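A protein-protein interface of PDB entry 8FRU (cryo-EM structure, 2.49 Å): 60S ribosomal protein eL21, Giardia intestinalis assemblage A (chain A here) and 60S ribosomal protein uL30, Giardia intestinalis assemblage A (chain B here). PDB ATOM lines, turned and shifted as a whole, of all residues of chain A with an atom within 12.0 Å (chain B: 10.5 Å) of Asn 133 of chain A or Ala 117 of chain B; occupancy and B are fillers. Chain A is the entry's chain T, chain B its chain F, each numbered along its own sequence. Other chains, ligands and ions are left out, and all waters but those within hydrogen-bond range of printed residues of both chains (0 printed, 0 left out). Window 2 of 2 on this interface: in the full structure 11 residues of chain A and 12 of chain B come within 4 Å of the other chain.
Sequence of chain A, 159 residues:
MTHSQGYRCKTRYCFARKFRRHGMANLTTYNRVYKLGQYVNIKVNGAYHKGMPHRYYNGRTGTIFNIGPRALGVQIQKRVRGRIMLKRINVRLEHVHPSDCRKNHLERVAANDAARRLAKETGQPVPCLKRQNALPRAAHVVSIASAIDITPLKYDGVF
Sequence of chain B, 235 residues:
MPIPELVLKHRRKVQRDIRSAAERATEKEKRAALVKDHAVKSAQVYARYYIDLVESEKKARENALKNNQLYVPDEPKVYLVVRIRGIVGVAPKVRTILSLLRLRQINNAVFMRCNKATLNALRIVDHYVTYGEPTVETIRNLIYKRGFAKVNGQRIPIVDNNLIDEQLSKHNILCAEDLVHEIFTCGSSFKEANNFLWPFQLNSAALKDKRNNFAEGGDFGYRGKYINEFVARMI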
ATOM      1  N   ASN A 104     -25.386   1.414  -5.830  1.00  0.00           N
ATOM      2  CA  ASN A 104     -26.000   1.936  -7.045  1.00  0.00           C
ATOM      3  C   ASN A 104     -25.337   1.360  -8.291  1.00  0.00           C
ATOM      4  O   ASN A 104     -26.021   0.963  -9.239  1.00  0.00           O
ATOM      5  CB  ASN A 104     -25.930   3.464  -7.035  1.00  0.00           C
ATOM      6  CG  ASN A 104     -26.514   4.089  -8.283  1.00  0.00           C
ATOM      7  OD1 ASN A 104     -25.785   4.492  -9.189  1.00  0.00           O
ATOM      8  ND2 ASN A 104     -27.833   4.183  -8.335  1.00  0.00           N
ATOM      9  N   ARG A 108     -27.061  -1.055 -11.087  1.00  0.00           N
ATOM     10  CA  ARG A 108     -27.050  -0.665 -12.493  1.00  0.00           C
ATOM     11  C   ARG A 108     -26.476  -1.768 -13.372  1.00  0.00           C
ATOM     12  O   ARG A 108     -27.008  -2.046 -14.450  1.00  0.00           O
ATOM     13  CB  ARG A 108     -26.269   0.634 -12.681  1.00  0.00           C
ATOM     14  CG  ARG A 108     -27.130   1.875 -12.584  1.00  0.00           C
ATOM     15  CD  ARG A 108     -26.345   3.140 -12.866  1.00  0.00           C
ATOM     16  NE  ARG A 108     -25.308   2.945 -13.872  1.00  0.00           N
ATOM     17  CZ  ARG A 108     -25.517   2.946 -15.180  1.00  0.00           C
ATOM     18  NH1 ARG A 108     -26.720   3.136 -15.687  1.00  0.00           N
ATOM     19  NH2 ARG A 108     -24.489   2.754 -15.998  1.00  0.00           N
ATOM     20  N   CYS A 128     -31.491   2.609 -24.547  1.00  0.00           N
ATOM     21  CA  CYS A 128     -30.254   3.240 -24.112  1.00  0.00           C
ATOM     22  C   CYS A 128     -30.001   2.883 -22.653  1.00  0.00           C
ATOM     23  O   CYS A 128     -30.853   3.123 -21.791  1.00  0.00           O
ATOM     24  CB  CYS A 128     -30.323   4.753 -24.297  1.00  0.00           C
ATOM     25  SG  CYS A 128     -28.712   5.572 -24.444  1.00  0.00           S
ATOM     26  N   LEU A 129     -28.833   2.305 -22.378  1.00  0.00           N
ATOM     27  CA  LEU A 129     -28.450   1.903 -21.032  1.00  0.00           C
ATOM     28  C   LEU A 129     -27.471   2.881 -20.395  1.00  0.00           C
ATOM     29  O   LEU A 129     -26.657   2.489 -19.553  1.00  0.00           O
ATOM     30  CB  LEU A 129     -27.862   0.494 -21.052  1.00  0.00           C
ATOM     31  CG  LEU A 129     -28.791  -0.591 -21.590  1.00  0.00           C
ATOM     32  CD1 LEU A 129     -28.158  -1.959 -21.435  1.00  0.00           C
ATOM     33  CD2 LEU A 129     -30.144  -0.530 -20.902  1.00  0.00           C
ATOM     34  N   LYS A 130     -27.534   4.149 -20.786  1.00  0.00           N
ATOM     35  CA  LYS A 130     -26.676   5.189 -20.247  1.00  0.00           C
ATOM     36  C   LYS A 130     -27.511   6.178 -19.453  1.00  0.00           C
ATOM     37  O   LYS A 130     -28.584   6.594 -19.898  1.00  0.00           O
ATOM     38  CB  LYS A 130     -25.931   5.921 -21.362  1.00  0.00           C
ATOM     39  CG  LYS A 130     -24.924   5.061 -22.092  1.00  0.00           C
ATOM     40  CD  LYS A 130     -24.325   5.798 -23.273  1.00  0.00           C
ATOM     41  CE  LYS A 130     -23.798   7.150 -22.861  1.00  0.00           C
ATOM     42  NZ  LYS A 130     -22.600   7.535 -23.655  1.00  0.00           N
ATOM     43  N   ARG A 131     -27.022   6.549 -18.276  1.00  0.00           N
ATOM     44  CA  ARG A 131     -27.680   7.601 -17.520  1.00  0.00           C
ATOM     45  C   ARG A 131     -27.673   8.895 -18.320  1.00  0.00           C
ATOM     46  O   ARG A 131     -26.737   9.187 -19.066  1.00  0.00           O
ATOM     47  CB  ARG A 131     -26.990   7.822 -16.176  1.00  0.00           C
ATOM     48  CG  ARG A 131     -26.956   6.608 -15.291  1.00  0.00           C
ATOM     49  CD  ARG A 131     -26.020   6.810 -14.127  1.00  0.00           C
ATOM     50  NE  ARG A 131     -24.634   6.660 -14.539  1.00  0.00           N
ATOM     51  CZ  ARG A 131     -23.591   6.967 -13.785  1.00  0.00           C
ATOM     52  NH1 ARG A 131     -23.739   7.432 -12.559  1.00  0.00           N
ATOM     53  NH2 ARG A 131     -22.369   6.793 -14.271  1.00  0.00           N
ATOM     54  N   GLN A 132     -28.738   9.669 -18.168  1.00  0.00           N
ATOM     55  CA  GLN A 132     -28.850  10.974 -18.795  1.00  0.00           C
ATOM     56  C   GLN A 132     -28.984  12.027 -17.710  1.00  0.00           C
ATOM     57  O   GLN A 132     -29.758  11.853 -16.765  1.00  0.00           O
ATOM     58  CB  GLN A 132     -30.050  11.036 -19.740  1.00  0.00           C
ATOM     59  CG  GLN A 132     -29.940  10.124 -20.942  1.00  0.00           C
ATOM     60  CD  GLN A 132     -29.090  10.710 -22.041  1.00  0.00           C
ATOM     61  OE1 GLN A 132     -27.862  10.643 -21.995  1.00  0.00           O
ATOM     62  NE2 GLN A 132     -29.739  11.293 -23.045  1.00  0.00           N
ATOM     63  N   ASN A 133     -28.221  13.106 -17.836  1.00  0.00           N
ATOM     64  CA  ASN A 133     -28.476  14.279 -17.016  1.00  0.00           C
ATOM     65  C   ASN A 133     -29.758  14.947 -17.491  1.00  0.00           C
ATOM     66  O   ASN A 133     -30.044  14.986 -18.690  1.00  0.00           O
ATOM     67  CB  ASN A 133     -27.299  15.248 -17.087  1.00  0.00           C
ATOM     68  CG  ASN A 133     -25.975  14.579 -16.786  1.00  0.00           C
ATOM     69  OD1 ASN A 133     -25.705  14.200 -15.651  1.00  0.00           O
ATOM     70  ND2 ASN A 133     -25.141  14.434 -17.802  1.00  0.00           N
ATOM     71  N   ALA A 134     -30.542  15.456 -16.544  1.00  0.00           N
ATOM     72  CA  ALA A 134     -31.881  15.951 -16.845  1.00  0.00           C
ATOM     73  C   ALA A 134     -31.881  16.845 -18.076  1.00  0.00           C
ATOM     74  O   ALA A 134     -31.203  17.875 -18.111  1.00  0.00           O
ATOM     75  CB  ALA A 134     -32.437  16.710 -15.643  1.00  0.00           C
ATOM     76  N   LEU A 135     -32.646  16.450 -19.080  1.00  0.00           N
ATOM     77  CA  LEU A 135     -32.786  17.200 -20.316  1.00  0.00           C
ATOM     78  C   LEU A 135     -33.880  18.249 -20.196  1.00  0.00           C
ATOM     79  O   LEU A 135     -34.734  18.178 -19.309  1.00  0.00           O
ATOM     80  CB  LEU A 135     -33.102  16.254 -21.468  1.00  0.00           C
ATOM     81  CG  LEU A 135     -32.010  15.242 -21.796  1.00  0.00           C
ATOM     82  CD1 LEU A 135     -32.605  13.891 -22.175  1.00  0.00           C
ATOM     83  CD2 LEU A 135     -31.128  15.779 -22.906  1.00  0.00           C
ATOM     84  N   PRO A 136     -33.871  19.250 -21.076  1.00  0.00           N
ATOM     85  CA  PRO A 136     -34.949  20.247 -21.072  1.00  0.00           C
ATOM     86  C   PRO A 136     -36.286  19.624 -21.440  1.00  0.00           C
ATOM     87  O   PRO A 136     -36.355  18.611 -22.137  1.00  0.00           O
ATOM     88  CB  PRO A 136     -34.495  21.264 -22.124  1.00  0.00           C
ATOM     89  CG  PRO A 136     -33.510  20.524 -22.966  1.00  0.00           C
ATOM     90  CD  PRO A 136     -32.814  19.588 -22.039  1.00  0.00           C
ATOM     91  N   ARG A 137     -37.357  20.251 -20.960  1.00  0.00           N
ATOM     92  CA  ARG A 137     -38.699  19.713 -21.116  1.00  0.00           C
ATOM     93  C   ARG A 137     -39.166  19.806 -22.567  1.00  0.00           C
ATOM     94  O   ARG A 137     -38.674  20.611 -23.361  1.00  0.00           O
ATOM     95  CB  ARG A 137     -39.675  20.448 -20.198  1.00  0.00           C
ATOM     96  CG  ARG A 137     -39.489  20.110 -18.732  1.00  0.00           C
ATOM     97  CD  ARG A 137     -40.513  20.788 -17.846  1.00  0.00           C
ATOM     98  NE  ARG A 137     -39.989  22.004 -17.236  1.00  0.00           N
ATOM     99  CZ  ARG A 137     -40.119  23.218 -17.751  1.00  0.00           C
ATOM    100  NH1 ARG A 137     -40.776  23.422 -18.880  1.00  0.00           N
ATOM    101  NH2 ARG A 137     -39.577  24.253 -17.115  1.00  0.00           N
ATOM    102  N   ALA A 138     -40.132  18.962 -22.905  1.00  0.00           N
ATOM    103  CA  ALA A 138     -40.659  18.854 -24.256  1.00  0.00           C
ATOM    104  C   ALA A 138     -41.968  19.629 -24.401  1.00  0.00           C
ATOM    105  O   ALA A 138     -42.542  20.127 -23.432  1.00  0.00           O
ATOM    106  CB  ALA A 138     -40.861  17.383 -24.632  1.00  0.00           C
ATOM    107  N   ILE B  97     -13.672  26.123 -14.583  1.00  0.00           N
ATOM    108  CA  ILE B  97     -14.897  25.971 -15.359  1.00  0.00           C
ATOM    109  C   ILE B  97     -14.772  26.670 -16.707  1.00  0.00           C
ATOM    110  O   ILE B  97     -15.189  26.134 -17.737  1.00  0.00           O
ATOM    111  CB  ILE B  97     -16.111  26.474 -14.560  1.00  0.00           C
ATOM    112  CG1 ILE B  97     -16.333  25.589 -13.340  1.00  0.00           C
ATOM    113  CG2 ILE B  97     -17.354  26.491 -15.424  1.00  0.00           C
ATOM    114  CD1 ILE B  97     -17.438  26.056 -12.445  1.00  0.00           C
ATOM    115  N   LEU B 100     -12.823  24.580 -19.060  1.00  0.00           N
ATOM    116  CA  LEU B 100     -13.533  23.424 -19.600  1.00  0.00           C
ATOM    117  C   LEU B 100     -14.536  23.797 -20.683  1.00  0.00           C
ATOM    118  O   LEU B 100     -14.951  22.922 -21.447  1.00  0.00           O
ATOM    119  CB  LEU B 100     -14.242  22.663 -18.483  1.00  0.00           C
ATOM    120  CG  LEU B 100     -13.346  21.957 -17.467  1.00  0.00           C
ATOM    121  CD1 LEU B 100     -14.173  21.129 -16.517  1.00  0.00           C
ATOM    122  CD2 LEU B 100     -12.311  21.097 -18.150  1.00  0.00           C
ATOM    123  N   LEU B 101     -14.946  25.060 -20.764  1.00  0.00           N
ATOM    124  CA  LEU B 101     -15.816  25.523 -21.836  1.00  0.00           C
ATOM    125  C   LEU B 101     -15.046  25.988 -23.064  1.00  0.00           C
ATOM    126  O   LEU B 101     -15.664  26.250 -24.098  1.00  0.00           O
ATOM    127  CB  LEU B 101     -16.703  26.672 -21.348  1.00  0.00           C
ATOM    128  CG  LEU B 101     -17.843  26.372 -20.380  1.00  0.00           C
ATOM    129  CD1 LEU B 101     -18.214  27.612 -19.595  1.00  0.00           C
ATOM    130  CD2 LEU B 101     -19.043  25.855 -21.130  1.00  0.00           C
ATOM    131  N   MET B 112     -22.898  25.248 -26.798  1.00  0.00           N
ATOM    132  CA  MET B 112     -22.998  24.450 -25.584  1.00  0.00           C
ATOM    133  C   MET B 112     -24.358  23.775 -25.517  1.00  0.00           C
ATOM    134  O   MET B 112     -25.386  24.446 -25.621  1.00  0.00           O
ATOM    135  CB  MET B 112     -22.789  25.326 -24.348  1.00  0.00           C
ATOM    136  CG  MET B 112     -22.685  24.566 -23.051  1.00  0.00           C
ATOM    137  SD  MET B 112     -22.624  25.669 -21.634  1.00  0.00           S
ATOM    138  CE  MET B 112     -24.307  25.550 -21.050  1.00  0.00           C
ATOM    139  N   ARG B 113     -24.360  22.459 -25.328  1.00  0.00           N
ATOM    140  CA  ARG B 113     -25.597  21.733 -25.089  1.00  0.00           C
ATOM    141  C   ARG B 113     -26.091  21.982 -23.668  1.00  0.00           C
ATOM    142  O   ARG B 113     -25.329  22.355 -22.775  1.00  0.00           O
ATOM    143  CB  ARG B 113     -25.402  20.238 -25.326  1.00  0.00           C
ATOM    144  CG  ARG B 113     -24.617  19.546 -24.245  1.00  0.00           C
ATOM    145  CD  ARG B 113     -24.218  18.145 -24.661  1.00  0.00           C
ATOM    146  NE  ARG B 113     -25.187  17.561 -25.578  1.00  0.00           N
ATOM    147  CZ  ARG B 113     -24.955  16.501 -26.337  1.00  0.00           C
ATOM    148  NH1 ARG B 113     -23.798  15.868 -26.305  1.00  0.00           N
ATOM    149  NH2 ARG B 113     -25.910  16.068 -27.153  1.00  0.00           N
ATOM    150  N   CYS B 114     -27.386  21.765 -23.460  1.00  0.00           N
ATOM    151  CA  CYS B 114     -28.045  22.093 -22.201  1.00  0.00           C
ATOM    152  C   CYS B 114     -28.449  20.821 -21.462  1.00  0.00           C
ATOM    153  O   CYS B 114     -29.253  20.036 -21.967  1.00  0.00           O
ATOM    154  CB  CYS B 114     -29.268  22.970 -22.456  1.00  0.00           C
ATOM    155  SG  CYS B 114     -28.919  24.611 -23.110  1.00  0.00           S
ATOM    156  N   ASN B 115     -27.883  20.621 -20.271  1.00  0.00           N
ATOM    157  CA  ASN B 115     -28.379  19.666 -19.289  1.00  0.00           C
ATOM    158  C   ASN B 115     -28.331  20.341 -17.928  1.00  0.00           C
ATOM    159  O   ASN B 115     -27.950  21.507 -17.807  1.00  0.00           O
ATOM    160  CB  ASN B 115     -27.560  18.371 -19.230  1.00  0.00           C
ATOM    161  CG  ASN B 115     -26.906  18.026 -20.533  1.00  0.00           C
ATOM    162  OD1 ASN B 115     -27.571  17.861 -21.549  1.00  0.00           O
ATOM    163  ND2 ASN B 115     -25.591  17.885 -20.510  1.00  0.00           N
ATOM    164  N   LYS B 116     -28.702  19.600 -16.888  1.00  0.00           N
ATOM    165  CA  LYS B 116     -28.517  20.120 -15.538  1.00  0.00           C
ATOM    166  C   LYS B 116     -27.035  20.245 -15.206  1.00  0.00           C
ATOM    167  O   LYS B 116     -26.610  21.212 -14.556  1.00  0.00           O
ATOM    168  CB  LYS B 116     -29.231  19.224 -14.532  1.00  0.00           C
ATOM    169  CG  LYS B 116     -29.530  19.911 -13.219  1.00  0.00           C
ATOM    170  CD  LYS B 116     -30.187  18.970 -12.245  1.00  0.00           C
ATOM    171  CE  LYS B 116     -30.212  19.560 -10.856  1.00  0.00           C
ATOM    172  NZ  LYS B 116     -30.967  18.694  -9.922  1.00  0.00           N
ATOM    173  N   ALA B 117     -26.232  19.291 -15.686  1.00  0.00           N
ATOM    174  CA  ALA B 117     -24.799  19.296 -15.419  1.00  0.00           C
ATOM    175  C   ALA B 117     -24.126  20.542 -15.984  1.00  0.00           C
ATOM    176  O   ALA B 117     -23.305  21.172 -15.312  1.00  0.00           O
ATOM    177  CB  ALA B 117     -24.164  18.032 -15.993  1.00  0.00           C
ATOM    178  N   THR B 118     -24.447  20.909 -17.224  1.00  0.00           N
ATOM    179  CA  THR B 118     -23.848  22.103 -17.807  1.00  0.00           C
ATOM    180  C   THR B 118     -24.482  23.377 -17.268  1.00  0.00           C
ATOM    181  O   THR B 118     -23.791  24.389 -17.092  1.00  0.00           O
ATOM    182  CB  THR B 118     -23.956  22.067 -19.333  1.00  0.00           C
ATOM    183  OG1 THR B 118     -25.327  21.956 -19.721  1.00  0.00           O
ATOM    184  CG2 THR B 118     -23.199  20.883 -19.891  1.00  0.00           C
ATOM    185  N   LEU B 119     -25.785  23.342 -16.997  1.00  0.00           N
ATOM    186  CA  LEU B 119     -26.480  24.540 -16.548  1.00  0.00           C
ATOM    187  C   LEU B 119     -25.975  25.004 -15.189  1.00  0.00           C
ATOM    188  O   LEU B 119     -25.806  26.207 -14.964  1.00  0.00           O
ATOM    189  CB  LEU B 119     -27.982  24.281 -16.512  1.00  0.00           C
ATOM    190  CG  LEU B 119     -28.678  24.443 -17.864  1.00  0.00           C
ATOM    191  CD1 LEU B 119     -30.138  24.052 -17.766  1.00  0.00           C
ATOM    192  CD2 LEU B 119     -28.538  25.859 -18.381  1.00  0.00           C
ATOM    193  N   ASN B 120     -25.723  24.074 -14.267  1.00  0.00           N
ATOM    194  CA  ASN B 120     -25.262  24.490 -12.945  1.00  0.00           C
ATOM    195  C   ASN B 120     -23.874  25.128 -12.999  1.00  0.00           C
ATOM    196  O   ASN B 120     -23.613  26.132 -12.319  1.00  0.00           O
ATOM    197  CB  ASN B 120     -25.301  23.300 -11.992  1.00  0.00           C
ATOM    198  CG  ASN B 120     -26.712  22.953 -11.573  1.00  0.00           C
ATOM    199  OD1 ASN B 120     -27.670  23.316 -12.246  1.00  0.00           O
ATOM    200  ND2 ASN B 120     -26.847  22.261 -10.457  1.00  0.00           N
ATOM    201  N   ALA B 121     -22.974  24.578 -13.813  1.00  0.00           N
ATOM    202  CA  ALA B 121     -21.664  25.198 -13.984  1.00  0.00           C
ATOM    203  C   ALA B 121     -21.785  26.584 -14.612  1.00  0.00           C
ATOM    204  O   ALA B 121     -21.102  27.535 -14.193  1.00  0.00           O
ATOM    205  CB  ALA B 121     -20.769  24.295 -14.825  1.00  0.00           C
ATOM    206  N   LEU B 122     -22.652  26.721 -15.615  1.00  0.00           N
ATOM    207  CA  LEU B 122     -22.873  28.035 -16.204  1.00  0.00           C
ATOM    208  C   LEU B 122     -23.363  29.027 -15.159  1.00  0.00           C
ATOM    209  O   LEU B 122     -22.948  30.194 -15.150  1.00  0.00           O
ATOM    210  CB  LEU B 122     -23.865  27.928 -17.358  1.00  0.00           C
ATOM    211  CG  LEU B 122     -23.806  29.036 -18.402  1.00  0.00           C
ATOM    212  CD1 LEU B 122     -22.394  29.226 -18.895  1.00  0.00           C
ATOM    213  CD2 LEU B 122     -24.728  28.708 -19.553  1.00  0.00           C
ATOM    214  N   ARG B 123     -24.252  28.588 -14.270  1.00  0.00           N
ATOM    215  CA  ARG B 123     -24.717  29.491 -13.226  1.00  0.00           C
ATOM    216  C   ARG B 123     -23.575  29.902 -12.311  1.00  0.00           C
ATOM    217  O   ARG B 123     -23.534  31.041 -11.834  1.00  0.00           O
ATOM    218  CB  ARG B 123     -25.844  28.856 -12.416  1.00  0.00           C
ATOM    219  CG  ARG B 123     -26.312  29.751 -11.276  1.00  0.00           C
ATOM    220  CD  ARG B 123     -27.507  29.185 -10.536  1.00  0.00           C
ATOM    221  NE  ARG B 123     -28.611  28.860 -11.429  1.00  0.00           N
ATOM    222  CZ  ARG B 123     -29.262  27.707 -11.417  1.00  0.00           C
ATOM    223  NH1 ARG B 123     -28.939  26.740 -10.576  1.00  0.00           N
ATOM    224  NH2 ARG B 123     -30.261  27.519 -12.272  1.00  0.00           N
ATOM    225  N   ILE B 124     -22.647  28.987 -12.034  1.00  0.00           N
ATOM    226  CA  ILE B 124     -21.524  29.362 -11.174  1.00  0.00           C
ATOM    227  C   ILE B 124     -20.645  30.418 -11.843  1.00  0.00           C
ATOM    228  O   ILE B 124     -20.098  31.296 -11.168  1.00  0.00           O
ATOM    229  CB  ILE B 124     -20.701  28.134 -10.757  1.00  0.00           C
ATOM    230  CG1 ILE B 124     -21.533  27.199  -9.887  1.00  0.00           C
ATOM    231  CG2 ILE B 124     -19.463  28.565 -10.008  1.00  0.00           C
ATOM    232  CD1 ILE B 124     -20.817  25.925  -9.532  1.00  0.00           C
ATOM    233  N   VAL B 125     -20.470  30.346 -13.163  1.00  0.00           N
ATOM    234  CA  VAL B 125     -19.589  31.308 -13.837  1.00  0.00           C
ATOM    235  C   VAL B 125     -20.351  32.501 -14.410  1.00  0.00           C
ATOM    236  O   VAL B 125     -19.770  33.303 -15.139  1.00  0.00           O
ATOM    237  CB  VAL B 125     -18.742  30.646 -14.936  1.00  0.00           C
ATOM    238  CG1 VAL B 125     -17.658  29.793 -14.327  1.00  0.00           C
ATOM    239  CG2 VAL B 125     -19.614  29.848 -15.877  1.00  0.00           C
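Asn 133 of chain A touches just these residues of chain B: Asn 115 and Ala 117. Of chain A, only Asn 133 (3.98 Å) comes within 4 Å of Ala 117 of chain B. Of chain B, only Asn 115 and Lys 116 come within 4 Å of Ala 134 of chain A. No residue of chain B comes within 4 Å of Leu 135 of chain A. Asn 115 of chain B touches two residues of chain A. Lys 116 of chain B touches just one residue of chain A: Ala 134. No residue of chain A comes within 4 Å of Thr 118 of chain B. No residue of chain A comes within 4 Å of Leu 119 of chain B. No residue of chain A comes within 4 Å of Asn 120 of chain B. Printed residues of chain A within 4 Å of Cys 114 of chain B: Pro 136. Of the printed residues of chain B, Pro 136 of chain A touches Cys 114 (3.6 Å). The nearest residue of chain B that does not touch Asn 133 of chain A is Lys 116 of chain B (4.6 Å). The nearest residue of chain A that does not touch Ala 117 of chain B is Ala 134 of chain A (5.7 Å).
CB of Asn 133 of chain A touches CB of Asn 115 of chain B, at 3.8 Å. Asn 133 of chain A touches Ala 117 of chain B (CG to CB, 3.98 Å). Ala 134 of chain A touches Asn 115 of chain B. CD of Pro 136 of chain A touches O of Cys 114 of chain B, at 3.6 Å.
The backbone carbonyl oxygen of Ala 134 of chain A is in hydrogen-bond range of the backbone NH of Lys 116 of chain B.
Of the 13 printed residues of chain A, 3 touch a printed residue of chain B. Printed residues of chain A that touch a printed residue of chain B: Asn 133, Ala 134 and Pro 136. Hydrophobic or aromatic side chains of chain A that line the printed part of chain B: Pro 136. Among the printed residues, 5 pairs touch across the chains.
O of Lys 116 of chain B lies close to OD1 of Asn 120 of chain B (3.3 Å). The backbone NH (N) of Asn 115 of chain B lies within hydrogen-bond range of the side-chain hydroxyl (OG1) of Thr 118 of chain B.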
